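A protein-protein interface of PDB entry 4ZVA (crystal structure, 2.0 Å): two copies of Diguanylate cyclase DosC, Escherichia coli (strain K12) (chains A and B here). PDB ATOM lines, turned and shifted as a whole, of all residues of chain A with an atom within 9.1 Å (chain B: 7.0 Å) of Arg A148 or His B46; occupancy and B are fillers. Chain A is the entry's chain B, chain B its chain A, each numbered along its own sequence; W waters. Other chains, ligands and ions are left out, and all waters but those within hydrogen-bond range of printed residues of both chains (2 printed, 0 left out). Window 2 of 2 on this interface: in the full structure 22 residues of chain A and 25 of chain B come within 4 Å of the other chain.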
ATOM      1  N   ALA A   2      12.558  17.803  -6.996  1.00  0.00           N
ATOM      2  CA  ALA A   2      13.036  17.103  -5.809  1.00  0.00           C
ATOM      3  C   ALA A   2      13.603  15.730  -6.163  1.00  0.00           C
ATOM      4  O   ALA A   2      14.548  15.257  -5.530  1.00  0.00           O
ATOM      5  CB  ALA A   2      11.916  16.966  -4.790  1.00  0.00           C
ATOM      6  N   MET A   3      13.018  15.097  -7.176  1.00  0.00           N
ATOM      7  CA  MET A   3      13.481  13.795  -7.643  1.00  0.00           C
ATOM      8  C   MET A   3      14.858  13.908  -8.285  1.00  0.00           C
ATOM      9  O   MET A   3      15.707  13.031  -8.114  1.00  0.00           O
ATOM     10  CB  MET A   3      12.485  13.187  -8.634  1.00  0.00           C
ATOM     11  CG  MET A   3      11.183  12.727  -8.002  1.00  0.00           C
ATOM     12  SD  MET A   3      11.445  11.543  -6.664  1.00  0.00           S
ATOM     13  CE  MET A   3      12.266  10.212  -7.535  1.00  0.00           C
ATOM     14  N   GLU A   6      17.532  14.189  -5.630  1.00  0.00           N
ATOM     15  CA  GLU A   6      17.769  12.913  -4.962  1.00  0.00           C
ATOM     16  C   GLU A   6      18.569  11.958  -5.846  1.00  0.00           C
ATOM     17  O   GLU A   6      19.495  11.296  -5.378  1.00  0.00           O
ATOM     18  CB  GLU A   6      16.451  12.260  -4.549  1.00  0.00           C
ATOM     19  CG  GLU A   6      16.626  10.845  -4.027  1.00  0.00           C
ATOM     20  CD  GLU A   6      15.695  10.517  -2.878  1.00  0.00           C
ATOM     21  OE1 GLU A   6      14.505  10.888  -2.947  1.00  0.00           O
ATOM     22  OE2 GLU A   6      16.159   9.891  -1.902  1.00  0.00           O
ATOM     23  N   ILE A  83      15.567  11.291 -16.549  1.00  0.00           N
ATOM     24  CA  ILE A  83      14.241  11.687 -16.088  1.00  0.00           C
ATOM     25  C   ILE A  83      13.264  11.827 -17.257  1.00  0.00           C
ATOM     26  O   ILE A  83      12.133  11.344 -17.187  1.00  0.00           O
ATOM     27  CB  ILE A  83      14.293  13.007 -15.293  1.00  0.00           C
ATOM     28  CG1 ILE A  83      14.986  12.785 -13.945  1.00  0.00           C
ATOM     29  CG2 ILE A  83      12.893  13.558 -15.064  1.00  0.00           C
ATOM     30  CD1 ILE A  83      15.286  14.060 -13.194  1.00  0.00           C
ATOM     31  N   GLN A  86      12.043   8.445 -18.537  1.00  0.00           N
ATOM     32  CA  GLN A  86      10.987   7.842 -17.730  1.00  0.00           C
ATOM     33  C   GLN A  86       9.626   8.430 -18.093  1.00  0.00           C
ATOM     34  O   GLN A  86       8.626   7.711 -18.135  1.00  0.00           O
ATOM     35  CB  GLN A  86      11.262   8.035 -16.236  1.00  0.00           C
ATOM     36  CG  GLN A  86      12.687   7.708 -15.811  1.00  0.00           C
ATOM     37  CD  GLN A  86      13.181   6.383 -16.358  1.00  0.00           C
ATOM     38  OE1 GLN A  86      12.457   5.387 -16.364  1.00  0.00           O
ATOM     39  NE2 GLN A  86      14.423   6.368 -16.829  1.00  0.00           N
ATOM     40  N   HIS A  87       9.593   9.733 -18.358  1.00  0.00           N
ATOM     41  CA  HIS A  87       8.374  10.383 -18.831  1.00  0.00           C
ATOM     42  C   HIS A  87       7.934   9.782 -20.162  1.00  0.00           C
ATOM     43  O   HIS A  87       6.755   9.497 -20.364  1.00  0.00           O
ATOM     44  CB  HIS A  87       8.580  11.894 -18.982  1.00  0.00           C
ATOM     45  CG  HIS A  87       8.526  12.649 -17.689  1.00  0.00           C
ATOM     46  ND1 HIS A  87       9.591  12.711 -16.816  1.00  0.00           N
ATOM     47  CD2 HIS A  87       7.534  13.378 -17.124  1.00  0.00           C
ATOM     48  CE1 HIS A  87       9.257  13.444 -15.769  1.00  0.00           C
ATOM     49  NE2 HIS A  87       8.014  13.861 -15.931  1.00  0.00           N
ATOM     50  N   ALA A  90       6.546   6.350 -19.650  1.00  0.00           N
ATOM     51  CA  ALA A  90       5.231   6.484 -19.030  1.00  0.00           C
ATOM     52  C   ALA A  90       4.164   6.790 -20.077  1.00  0.00           C
ATOM     53  O   ALA A  90       3.074   6.216 -20.050  1.00  0.00           O
ATOM     54  CB  ALA A  90       5.254   7.571 -17.963  1.00  0.00           C
ATOM     55  N   VAL A 100      -0.684   0.880 -13.860  1.00  0.00           N
ATOM     56  CA  VAL A 100       0.501   1.253 -13.096  1.00  0.00           C
ATOM     57  C   VAL A 100       1.010   0.102 -12.230  1.00  0.00           C
ATOM     58  O   VAL A 100       2.218  -0.078 -12.076  1.00  0.00           O
ATOM     59  CB  VAL A 100       0.223   2.477 -12.198  1.00  0.00           C
ATOM     60  CG1 VAL A 100       1.505   2.961 -11.535  1.00  0.00           C
ATOM     61  CG2 VAL A 100      -0.416   3.594 -13.008  1.00  0.00           C
ATOM     62  N   GLU A 104       4.614  -1.665 -12.066  1.00  0.00           N
ATOM     63  CA  GLU A 104       5.285  -1.859 -10.781  1.00  0.00           C
ATOM     64  C   GLU A 104       5.713  -3.307 -10.594  1.00  0.00           C
ATOM     65  O   GLU A 104       6.796  -3.581 -10.079  1.00  0.00           O
ATOM     66  CB  GLU A 104       4.376  -1.440  -9.625  1.00  0.00           C
ATOM     67  CG  GLU A 104       4.167   0.057  -9.493  1.00  0.00           C
ATOM     68  CD  GLU A 104       3.436   0.424  -8.215  1.00  0.00           C
ATOM     69  OE1 GLU A 104       3.124  -0.495  -7.427  1.00  0.00           O
ATOM     70  OE2 GLU A 104       3.175   1.624  -7.995  1.00  0.00           O
ATOM     71  N   ASP A 140      14.300   2.189  -7.973  1.00  0.00           N
ATOM     72  CA  ASP A 140      13.133   2.712  -7.267  1.00  0.00           C
ATOM     73  C   ASP A 140      12.921   4.189  -7.566  1.00  0.00           C
ATOM     74  O   ASP A 140      11.787   4.638  -7.721  1.00  0.00           O
ATOM     75  CB  ASP A 140      13.262   2.501  -5.758  1.00  0.00           C
ATOM     76  CG  ASP A 140      12.847   1.111  -5.331  1.00  0.00           C
ATOM     77  OD1 ASP A 140      12.238   0.392  -6.154  1.00  0.00           O
ATOM     78  OD2 ASP A 140      13.113   0.741  -4.169  1.00  0.00           O
ATOM     79  N   ILE A 141      14.013   4.945  -7.621  1.00  0.00           N
ATOM     80  CA  ILE A 141      13.925   6.364  -7.938  1.00  0.00           C
ATOM     81  C   ILE A 141      13.398   6.543  -9.359  1.00  0.00           C
ATOM     82  O   ILE A 141      12.560   7.407  -9.618  1.00  0.00           O
ATOM     83  CB  ILE A 141      15.296   7.063  -7.796  1.00  0.00           C
ATOM     84  CG1 ILE A 141      15.606   7.333  -6.325  1.00  0.00           C
ATOM     85  CG2 ILE A 141      15.325   8.369  -8.569  1.00  0.00           C
ATOM     86  CD1 ILE A 141      16.988   7.904  -6.093  1.00  0.00           C
ATOM     87  N   ALA A 142      13.851   5.683 -10.263  1.00  0.00           N
ATOM     88  CA  ALA A 142      13.395   5.735 -11.648  1.00  0.00           C
ATOM     89  C   ALA A 142      11.924   5.354 -11.733  1.00  0.00           C
ATOM     90  O   ALA A 142      11.165   5.953 -12.491  1.00  0.00           O
ATOM     91  CB  ALA A 142      14.235   4.822 -12.524  1.00  0.00           C
ATOM     92  N   MET A 143      11.522   4.366 -10.940  1.00  0.00           N
ATOM     93  CA  MET A 143      10.130   3.935 -10.933  1.00  0.00           C
ATOM     94  C   MET A 143       9.212   5.059 -10.466  1.00  0.00           C
ATOM     95  O   MET A 143       8.142   5.267 -11.038  1.00  0.00           O
ATOM     96  CB  MET A 143       9.941   2.699 -10.052  1.00  0.00           C
ATOM     97  CG  MET A 143       8.482   2.307  -9.886  1.00  0.00           C
ATOM     98  SD  MET A 143       8.244   0.688  -9.146  1.00  0.00           S
ATOM     99  CE  MET A 143       8.793   0.995  -7.469  1.00  0.00           C
ATOM    100  N   GLU A 144       9.632   5.788  -9.437  1.00  0.00           N
ATOM    101  CA  GLU A 144       8.818   6.879  -8.910  1.00  0.00           C
ATOM    102  C   GLU A 144       8.662   7.994  -9.941  1.00  0.00           C
ATOM    103  O   GLU A 144       7.575   8.541 -10.107  1.00  0.00           O
ATOM    104  CB  GLU A 144       9.412   7.432  -7.613  1.00  0.00           C
ATOM    105  CG  GLU A 144       8.587   8.558  -7.007  1.00  0.00           C
ATOM    106  CD  GLU A 144       9.038   8.937  -5.611  1.00  0.00           C
ATOM    107  OE1 GLU A 144       9.573   8.057  -4.905  1.00  0.00           O
ATOM    108  OE2 GLU A 144       8.848  10.107  -5.215  1.00  0.00           O
ATOM    109  N   VAL A 145       9.751   8.329 -10.627  1.00  0.00           N
ATOM    110  CA  VAL A 145       9.701   9.325 -11.692  1.00  0.00           C
ATOM    111  C   VAL A 145       8.723   8.896 -12.780  1.00  0.00           C
ATOM    112  O   VAL A 145       7.918   9.696 -13.257  1.00  0.00           O
ATOM    113  CB  VAL A 145      11.093   9.560 -12.319  1.00  0.00           C
ATOM    114  CG1 VAL A 145      10.991  10.491 -13.515  1.00  0.00           C
ATOM    115  CG2 VAL A 145      12.054  10.121 -11.283  1.00  0.00           C
ATOM    116  N   MET A 146       8.780   7.621 -13.147  1.00  0.00           N
ATOM    117  CA  MET A 146       7.918   7.094 -14.196  1.00  0.00           C
ATOM    118  C   MET A 146       6.456   7.097 -13.764  1.00  0.00           C
ATOM    119  O   MET A 146       5.584   7.527 -14.517  1.00  0.00           O
ATOM    120  CB  MET A 146       8.344   5.673 -14.581  1.00  0.00           C
ATOM    121  CG  MET A 146       7.594   5.102 -15.778  1.00  0.00           C
ATOM    122  SD  MET A 146       8.011   3.387 -16.153  1.00  0.00           S
ATOM    123  CE  MET A 146       9.773   3.515 -16.451  1.00  0.00           C
ATOM    124  N   THR A 147       6.190   6.629 -12.550  1.00  0.00           N
ATOM    125  CA  THR A 147       4.814   6.528 -12.085  1.00  0.00           C
ATOM    126  C   THR A 147       4.200   7.886 -11.753  1.00  0.00           C
ATOM    127  O   THR A 147       2.993   8.075 -11.899  1.00  0.00           O
ATOM    128  CB  THR A 147       4.712   5.629 -10.838  1.00  0.00           C
ATOM    129  OG1 THR A 147       5.628   6.091  -9.838  1.00  0.00           O
ATOM    130  CG2 THR A 147       5.043   4.189 -11.192  1.00  0.00           C
ATOM    131  N   ARG A 148       5.025   8.835 -11.317  1.00  0.00           N
ATOM    132  CA  ARG A 148       4.525  10.175 -11.025  1.00  0.00           C
ATOM    133  C   ARG A 148       4.492  11.033 -12.287  1.00  0.00           C
ATOM    134  O   ARG A 148       5.013  12.148 -12.304  1.00  0.00           O
ATOM    135  CB  ARG A 148       5.366  10.842  -9.931  1.00  0.00           C
ATOM    136  CG  ARG A 148       5.207  10.143  -8.583  1.00  0.00           C
ATOM    137  CD  ARG A 148       5.918  10.825  -7.423  1.00  0.00           C
ATOM    138  NE  ARG A 148       5.111  11.893  -6.843  1.00  0.00           N
ATOM    139  CZ  ARG A 148       5.447  12.577  -5.755  1.00  0.00           C
ATOM    140  NH1 ARG A 148       6.575  12.297  -5.116  1.00  0.00           N
ATOM    141  NH2 ARG A 148       4.649  13.533  -5.297  1.00  0.00           N
ATOM    142  N   ALA A 149       3.865  10.510 -13.337  1.00  0.00           N
ATOM    143  CA  ALA A 149       3.781  11.214 -14.612  1.00  0.00           C
ATOM    144  C   ALA A 149       2.470  10.908 -15.327  1.00  0.00           C
ATOM    145  O   ALA A 149       1.666  11.806 -15.581  1.00  0.00           O
ATOM    146  CB  ALA A 149       4.966  10.848 -15.495  1.00  0.00           C
ATOM    147  N   VAL B  41       8.092  11.496   4.784  1.00  0.00           N
ATOM    148  CA  VAL B  41       6.858  11.528   4.007  1.00  0.00           C
ATOM    149  C   VAL B  41       6.155  12.882   4.135  1.00  0.00           C
ATOM    150  O   VAL B  41       5.630  13.414   3.155  1.00  0.00           O
ATOM    151  CB  VAL B  41       5.906  10.397   4.449  1.00  0.00           C
ATOM    152  CG1 VAL B  41       4.470  10.700   4.055  1.00  0.00           C
ATOM    153  CG2 VAL B  41       6.369   9.064   3.879  1.00  0.00           C
ATOM    154  N   ARG B  42       6.181  13.445   5.341  1.00  0.00           N
ATOM    155  CA  ARG B  42       5.566  14.743   5.622  1.00  0.00           C
ATOM    156  C   ARG B  42       6.120  15.860   4.738  1.00  0.00           C
ATOM    157  O   ARG B  42       5.421  16.833   4.447  1.00  0.00           O
ATOM    158  CB  ARG B  42       5.759  15.114   7.095  1.00  0.00           C
ATOM    159  CG  ARG B  42       4.705  14.546   8.034  1.00  0.00           C
ATOM    160  CD  ARG B  42       3.492  15.454   8.139  1.00  0.00           C
ATOM    161  NE  ARG B  42       3.797  16.690   8.856  1.00  0.00           N
ATOM    162  CZ  ARG B  42       2.916  17.659   9.081  1.00  0.00           C
ATOM    163  NH1 ARG B  42       1.669  17.540   8.647  1.00  0.00           N
ATOM    164  NH2 ARG B  42       3.282  18.750   9.742  1.00  0.00           N
ATOM    165  N   ILE B  43       7.377  15.722   4.327  1.00  0.00           N
ATOM    166  CA  ILE B  43       8.028  16.717   3.480  1.00  0.00           C
ATOM    167  C   ILE B  43       7.303  16.866   2.143  1.00  0.00           C
ATOM    168  O   ILE B  43       7.162  17.972   1.622  1.00  0.00           O
ATOM    169  CB  ILE B  43       9.508  16.356   3.221  1.00  0.00           C
ATOM    170  CG1 ILE B  43      10.254  16.173   4.544  1.00  0.00           C
ATOM    171  CG2 ILE B  43      10.188  17.422   2.376  1.00  0.00           C
ATOM    172  CD1 ILE B  43      10.240  17.402   5.426  1.00  0.00           C
ATOM    173  N   ASP B  44       6.836  15.747   1.597  1.00  0.00           N
ATOM    174  CA  ASP B  44       6.098  15.763   0.339  1.00  0.00           C
ATOM    175  C   ASP B  44       4.766  16.485   0.522  1.00  0.00           C
ATOM    176  O   ASP B  44       3.947  16.081   1.347  1.00  0.00           O
ATOM    177  CB  ASP B  44       5.877  14.336  -0.173  1.00  0.00           C
ATOM    178  CG  ASP B  44       5.374  14.295  -1.609  1.00  0.00           C
ATOM    179  OD1 ASP B  44       4.410  15.017  -1.941  1.00  0.00           O
ATOM    180  OD2 ASP B  44       5.953  13.535  -2.414  1.00  0.00           O
ATOM    181  N   PRO B  45       4.550  17.560  -0.254  1.00  0.00           N
ATOM    182  CA  PRO B  45       3.339  18.387  -0.180  1.00  0.00           C
ATOM    183  C   PRO B  45       2.063  17.597  -0.456  1.00  0.00           C
ATOM    184  O   PRO B  45       1.047  17.821   0.201  1.00  0.00           O
ATOM    185  CB  PRO B  45       3.568  19.439  -1.270  1.00  0.00           C
ATOM    186  CG  PRO B  45       5.046  19.487  -1.449  1.00  0.00           C
ATOM    187  CD  PRO B  45       5.512  18.081  -1.240  1.00  0.00           C
ATOM    188  N   HIS B  46       2.121  16.682  -1.418  1.00  0.00           N
ATOM    189  CA  HIS B  46       0.955  15.889  -1.789  1.00  0.00           C
ATOM    190  C   HIS B  46       0.615  14.852  -0.723  1.00  0.00           C
ATOM    191  O   HIS B  46      -0.509  14.355  -0.665  1.00  0.00           O
ATOM    192  CB  HIS B  46       1.186  15.194  -3.132  1.00  0.00           C
ATOM    193  CG  HIS B  46       1.381  16.138  -4.277  1.00  0.00           C
ATOM    194  ND1 HIS B  46       0.336  16.801  -4.883  1.00  0.00           N
ATOM    195  CD2 HIS B  46       2.502  16.523  -4.934  1.00  0.00           C
ATOM    196  CE1 HIS B  46       0.804  17.558  -5.859  1.00  0.00           C
ATOM    197  NE2 HIS B  46       2.115  17.406  -5.911  1.00  0.00           N
ATOM    198  N   ALA B  47       1.589  14.531   0.120  1.00  0.00           N
ATOM    199  CA  ALA B  47       1.397  13.534   1.166  1.00  0.00           C
ATOM    200  C   ALA B  47       1.108  14.198   2.506  1.00  0.00           C
ATOM    201  O   ALA B  47       0.477  13.604   3.381  1.00  0.00           O
ATOM    202  CB  ALA B  47       2.618  12.634   1.273  1.00  0.00           C
ATOM    203  N   GLU B  48       1.572  15.435   2.658  1.00  0.00           N
ATOM    204  CA  GLU B  48       1.399  16.181   3.899  1.00  0.00           C
ATOM    205  C   GLU B  48      -0.079  16.444   4.175  1.00  0.00           C
ATOM    206  O   GLU B  48      -0.491  16.579   5.328  1.00  0.00           O
ATOM    207  CB  GLU B  48       2.183  17.498   3.837  1.00  0.00           C
ATOM    208  CG  GLU B  48       2.284  18.249   5.159  1.00  0.00           C
ATOM    209  CD  GLU B  48       1.104  19.167   5.409  1.00  0.00           C
ATOM    210  OE1 GLU B  48       0.396  19.505   4.437  1.00  0.00           O
ATOM    211  OE2 GLU B  48       0.883  19.548   6.578  1.00  0.00           O
ATOM    212  N   GLU B  49      -0.870  16.509   3.110  1.00  0.00           N
ATOM    213  CA  GLU B  49      -2.304  16.753   3.217  1.00  0.00           C
ATOM    214  C   GLU B  49      -3.009  15.678   4.043  1.00  0.00           C
ATOM    215  O   GLU B  49      -3.928  15.973   4.808  1.00  0.00           O
ATOM    216  CB  GLU B  49      -2.931  16.828   1.824  1.00  0.00           C
ATOM    217  CG  GLU B  49      -4.421  17.122   1.825  1.00  0.00           C
ATOM    218  CD  GLU B  49      -5.039  16.995   0.446  1.00  0.00           C
ATOM    219  OE1 GLU B  49      -4.299  16.686  -0.511  1.00  0.00           O
ATOM    220  OE2 GLU B  49      -6.264  17.204   0.321  1.00  0.00           O
ATOM    221  N   PHE B  50      -2.564  14.434   3.894  1.00  0.00           N
ATOM    222  CA  PHE B  50      -3.209  13.306   4.558  1.00  0.00           C
ATOM    223  C   PHE B  50      -2.738  13.145   6.001  1.00  0.00           C
ATOM    224  O   PHE B  50      -3.246  12.302   6.738  1.00  0.00           O
ATOM    225  CB  PHE B  50      -2.951  12.015   3.780  1.00  0.00           C
ATOM    226  CG  PHE B  50      -3.381  12.078   2.343  1.00  0.00           C
ATOM    227  CD1 PHE B  50      -4.708  11.899   1.995  1.00  0.00           C
ATOM    228  CD2 PHE B  50      -2.456  12.316   1.339  1.00  0.00           C
ATOM    229  CE1 PHE B  50      -5.108  11.956   0.673  1.00  0.00           C
ATOM    230  CE2 PHE B  50      -2.850  12.373   0.015  1.00  0.00           C
ATOM    231  CZ  PHE B  50      -4.177  12.192  -0.319  1.00  0.00           C
ATOM    232  N   ILE B  98      -5.802   8.448  -1.116  1.00  0.00           N
ATOM    233  CA  ILE B  98      -4.358   8.570  -1.289  1.00  0.00           C
ATOM    234  C   ILE B  98      -3.906   7.965  -2.616  1.00  0.00           C
ATOM    235  O   ILE B  98      -4.124   6.780  -2.867  1.00  0.00           O
ATOM    236  CB  ILE B  98      -3.605   7.887  -0.139  1.00  0.00           C
ATOM    237  CG1 ILE B  98      -4.111   8.412   1.204  1.00  0.00           C
ATOM    238  CG2 ILE B  98      -2.105   8.098  -0.283  1.00  0.00           C
ATOM    239  CD1 ILE B  98      -3.524   7.701   2.389  1.00  0.00           C
ATOM    240  N   PRO B  99      -3.266   8.784  -3.468  1.00  0.00           N
ATOM    241  CA  PRO B  99      -2.791   8.365  -4.792  1.00  0.00           C
ATOM    242  C   PRO B  99      -1.787   7.217  -4.722  1.00  0.00           C
ATOM    243  O   PRO B  99      -1.019   7.128  -3.764  1.00  0.00           O
ATOM    244  CB  PRO B  99      -2.128   9.632  -5.344  1.00  0.00           C
ATOM    245  CG  PRO B  99      -2.744  10.751  -4.581  1.00  0.00           C
ATOM    246  CD  PRO B  99      -2.988  10.206  -3.210  1.00  0.00           C
ATOM    247  N   GLU B 101       0.873   6.674  -6.432  1.00  0.00           N
ATOM    248  CA  GLU B 101       2.258   7.124  -6.508  1.00  0.00           C
ATOM    249  C   GLU B 101       2.709   7.743  -5.188  1.00  0.00           C
ATOM    250  O   GLU B 101       3.906   7.849  -4.920  1.00  0.00           O
ATOM    251  CB  GLU B 101       2.444   8.122  -7.655  1.00  0.00           C
ATOM    252  CG  GLU B 101       1.831   9.492  -7.421  1.00  0.00           C
ATOM    253  CD  GLU B 101       0.358   9.547  -7.778  1.00  0.00           C
ATOM    254  OE1 GLU B 101      -0.182   8.525  -8.252  1.00  0.00           O
ATOM    255  OE2 GLU B 101      -0.260  10.615  -7.591  1.00  0.00           O
ATOM    256  N   ILE B 102       1.749   8.147  -4.364  1.00  0.00           N
ATOM    257  CA  ILE B 102       2.061   8.652  -3.033  1.00  0.00           C
ATOM    258  C   ILE B 102       2.387   7.484  -2.107  1.00  0.00           C
ATOM    259  O   ILE B 102       3.319   7.554  -1.304  1.00  0.00           O
ATOM    260  CB  ILE B 102       0.896   9.484  -2.456  1.00  0.00           C
ATOM    261  CG1 ILE B 102       0.721  10.770  -3.262  1.00  0.00           C
ATOM    262  CG2 ILE B 102       1.144   9.829  -1.001  1.00  0.00           C
ATOM    263  CD1 ILE B 102       1.941  11.663  -3.239  1.00  0.00           C
ATOM    264  N   GLU B 104       3.422   4.475  -3.209  1.00  0.00           N
ATOM    265  CA  GLU B 104       4.665   3.933  -3.749  1.00  0.00           C
ATOM    266  C   GLU B 104       5.871   4.712  -3.235  1.00  0.00           C
ATOM    267  O   GLU B 104       6.904   4.129  -2.904  1.00  0.00           O
ATOM    268  CB  GLU B 104       4.644   3.953  -5.279  1.00  0.00           C
ATOM    269  CG  GLU B 104       5.911   3.402  -5.913  1.00  0.00           C
ATOM    270  CD  GLU B 104       6.003   3.701  -7.396  1.00  0.00           C
ATOM    271  OE1 GLU B 104       5.191   3.152  -8.171  1.00  0.00           O
ATOM    272  OE2 GLU B 104       6.891   4.489  -7.785  1.00  0.00           O
ATOM    273  N   MET B 105       5.726   6.032  -3.169  1.00  0.00           N
ATOM    274  CA  MET B 105       6.763   6.903  -2.630  1.00  0.00           C
ATOM    275  C   MET B 105       7.053   6.570  -1.169  1.00  0.00           C
ATOM    276  O   MET B 105       8.197   6.649  -0.721  1.00  0.00           O
ATOM    277  CB  MET B 105       6.352   8.372  -2.771  1.00  0.00           C
ATOM    278  CG  MET B 105       7.374   9.373  -2.248  1.00  0.00           C
ATOM    279  SD  MET B 105       7.151   9.798  -0.506  1.00  0.00           S
ATOM    280  CE  MET B 105       5.541  10.575  -0.550  1.00  0.00           C
ATOM    281  N   ARG B 108       9.257   3.567  -1.050  1.00  0.00           N
ATOM    282  CA  ARG B 108      10.623   3.900  -1.431  1.00  0.00           C
ATOM    283  C   ARG B 108      11.359   4.522  -0.251  1.00  0.00           C
ATOM    284  O   ARG B 108      12.523   4.212  -0.001  1.00  0.00           O
ATOM    285  CB  ARG B 108      10.651   4.847  -2.631  1.00  0.00           C
ATOM    286  CG  ARG B 108      12.050   5.041  -3.203  1.00  0.00           C
ATOM    287  CD  ARG B 108      12.058   5.971  -4.405  1.00  0.00           C
ATOM    288  NE  ARG B 108      11.800   7.357  -4.036  1.00  0.00           N
ATOM    289  CZ  ARG B 108      12.710   8.167  -3.505  1.00  0.00           C
ATOM    290  NH1 ARG B 108      13.940   7.724  -3.279  1.00  0.00           N
ATOM    291  NH2 ARG B 108      12.392   9.418  -3.201  1.00  0.00           N
HETATM  292  O   HOH W   1       9.730   3.802  -6.002  1.00  0.00           O
HETATM  293  O   HOH W   2      10.219  11.259  -3.570  1.00  0.00           O
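The backbone carbonyl oxygen (O) of Met A143 is in hydrogen-bond range of the side-chain hydroxyl (OG1) of Thr A147 (2.9 Å). OE2 of Glu A144 is in salt-bridge range of NH1 of Arg A148 (3.2 Å). The side-chain carboxylate (OD1) of Asp B44 sits at hydrogen-bond distance from the backbone NH (N) of His B46 (2.9 Å). The backbone carbonyl oxygen of Glu A144 is in hydrogen-bond range of the side-chain hydroxyl of Thr A147, 3.1 Å away.
Glu B104 touches its own counterpart, Glu A104. Of the 13 pairs that touch across the chains among the printed residues, 1 has its exchanged pair printed and touching as well.
Among the printed residues, merely in contact across the chains: Asp A140 with Arg B108 (3.6 Å), Ile A141 with Arg B108 (3.5 Å), Met A143 with Glu B104 (3.4 Å), Glu A144 with Met B105 (3.4 Å), Arg A148 with His B46 (3.7 Å), Arg A148 with Glu B101 (3.5 Å) and Arg A148 with Ile B102 (3.9 Å).
Water W2 lies within hydrogen-bond range of OE2 of Glu A144, NH2 of Arg B108 and SD of Met A3. Water W1 lies within hydrogen-bond range of the backbone carbonyl oxygen (O) of Asp A140 (2.8 Å) and the side-chain carboxylate (OE2) of Glu B104 (3.4 Å).
Arg A148 touches four residues of chain B. Of chain A, only Arg A148 (3.7 Å) comes within 4 Å of His B46. No residue of chain A comes within 4 Å of Ala B47. Printed residues of chain A within 4 Å of Arg B108: Glu A6, Asp A140, Ile A141 and Glu A144. Of the printed residues of chain B, Glu A6 touches Arg B108 (2.6 Å). The nearest residue of chain B that does not touch Arg A148 is Met B105 (4.2 Å).
Of the 17 printed residues of chain B, 7 touch a printed residue of chain A. Hydrophobic or aromatic side chains of chain B within 4 Å of the printed part of chain A: His B46, Ile B102 and Met B105. Of the 19 printed residues of chain A, 8 touch a printed residue of chain B. Hydrophobic or aromatic side chains of chain A within 4 Å of the printed part of chain B: Ile A141 and Met A143. Along chain A the printed residues that touch a printed residue of chain B span positions 6 to 148.
OG1 of Thr A147 lies within hydrogen-bond range of OE2 of Glu B104 (2.9 Å). The side-chain carboxylate (OD2) of Asp B44 is in salt-bridge range of the guanidinium group (NH1) of Arg A148, at 3.0 Å. NH2 of Arg B108 is in salt-bridge range of OE1 of Glu A6, 2.6 Å away. The side-chain carboxylate of Glu B104 lies close to the side-chain carboxylate of Glu A104, at 2.5 Å. The side-chain carboxylate of Glu B104 lies close to the backbone NH of Glu A144 (3.5 Å). The side-chain carboxylate (OE1) of Glu A144 lies within salt-bridge range of the guanidinium group (NE) of Arg B108, at 2.5 Å.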
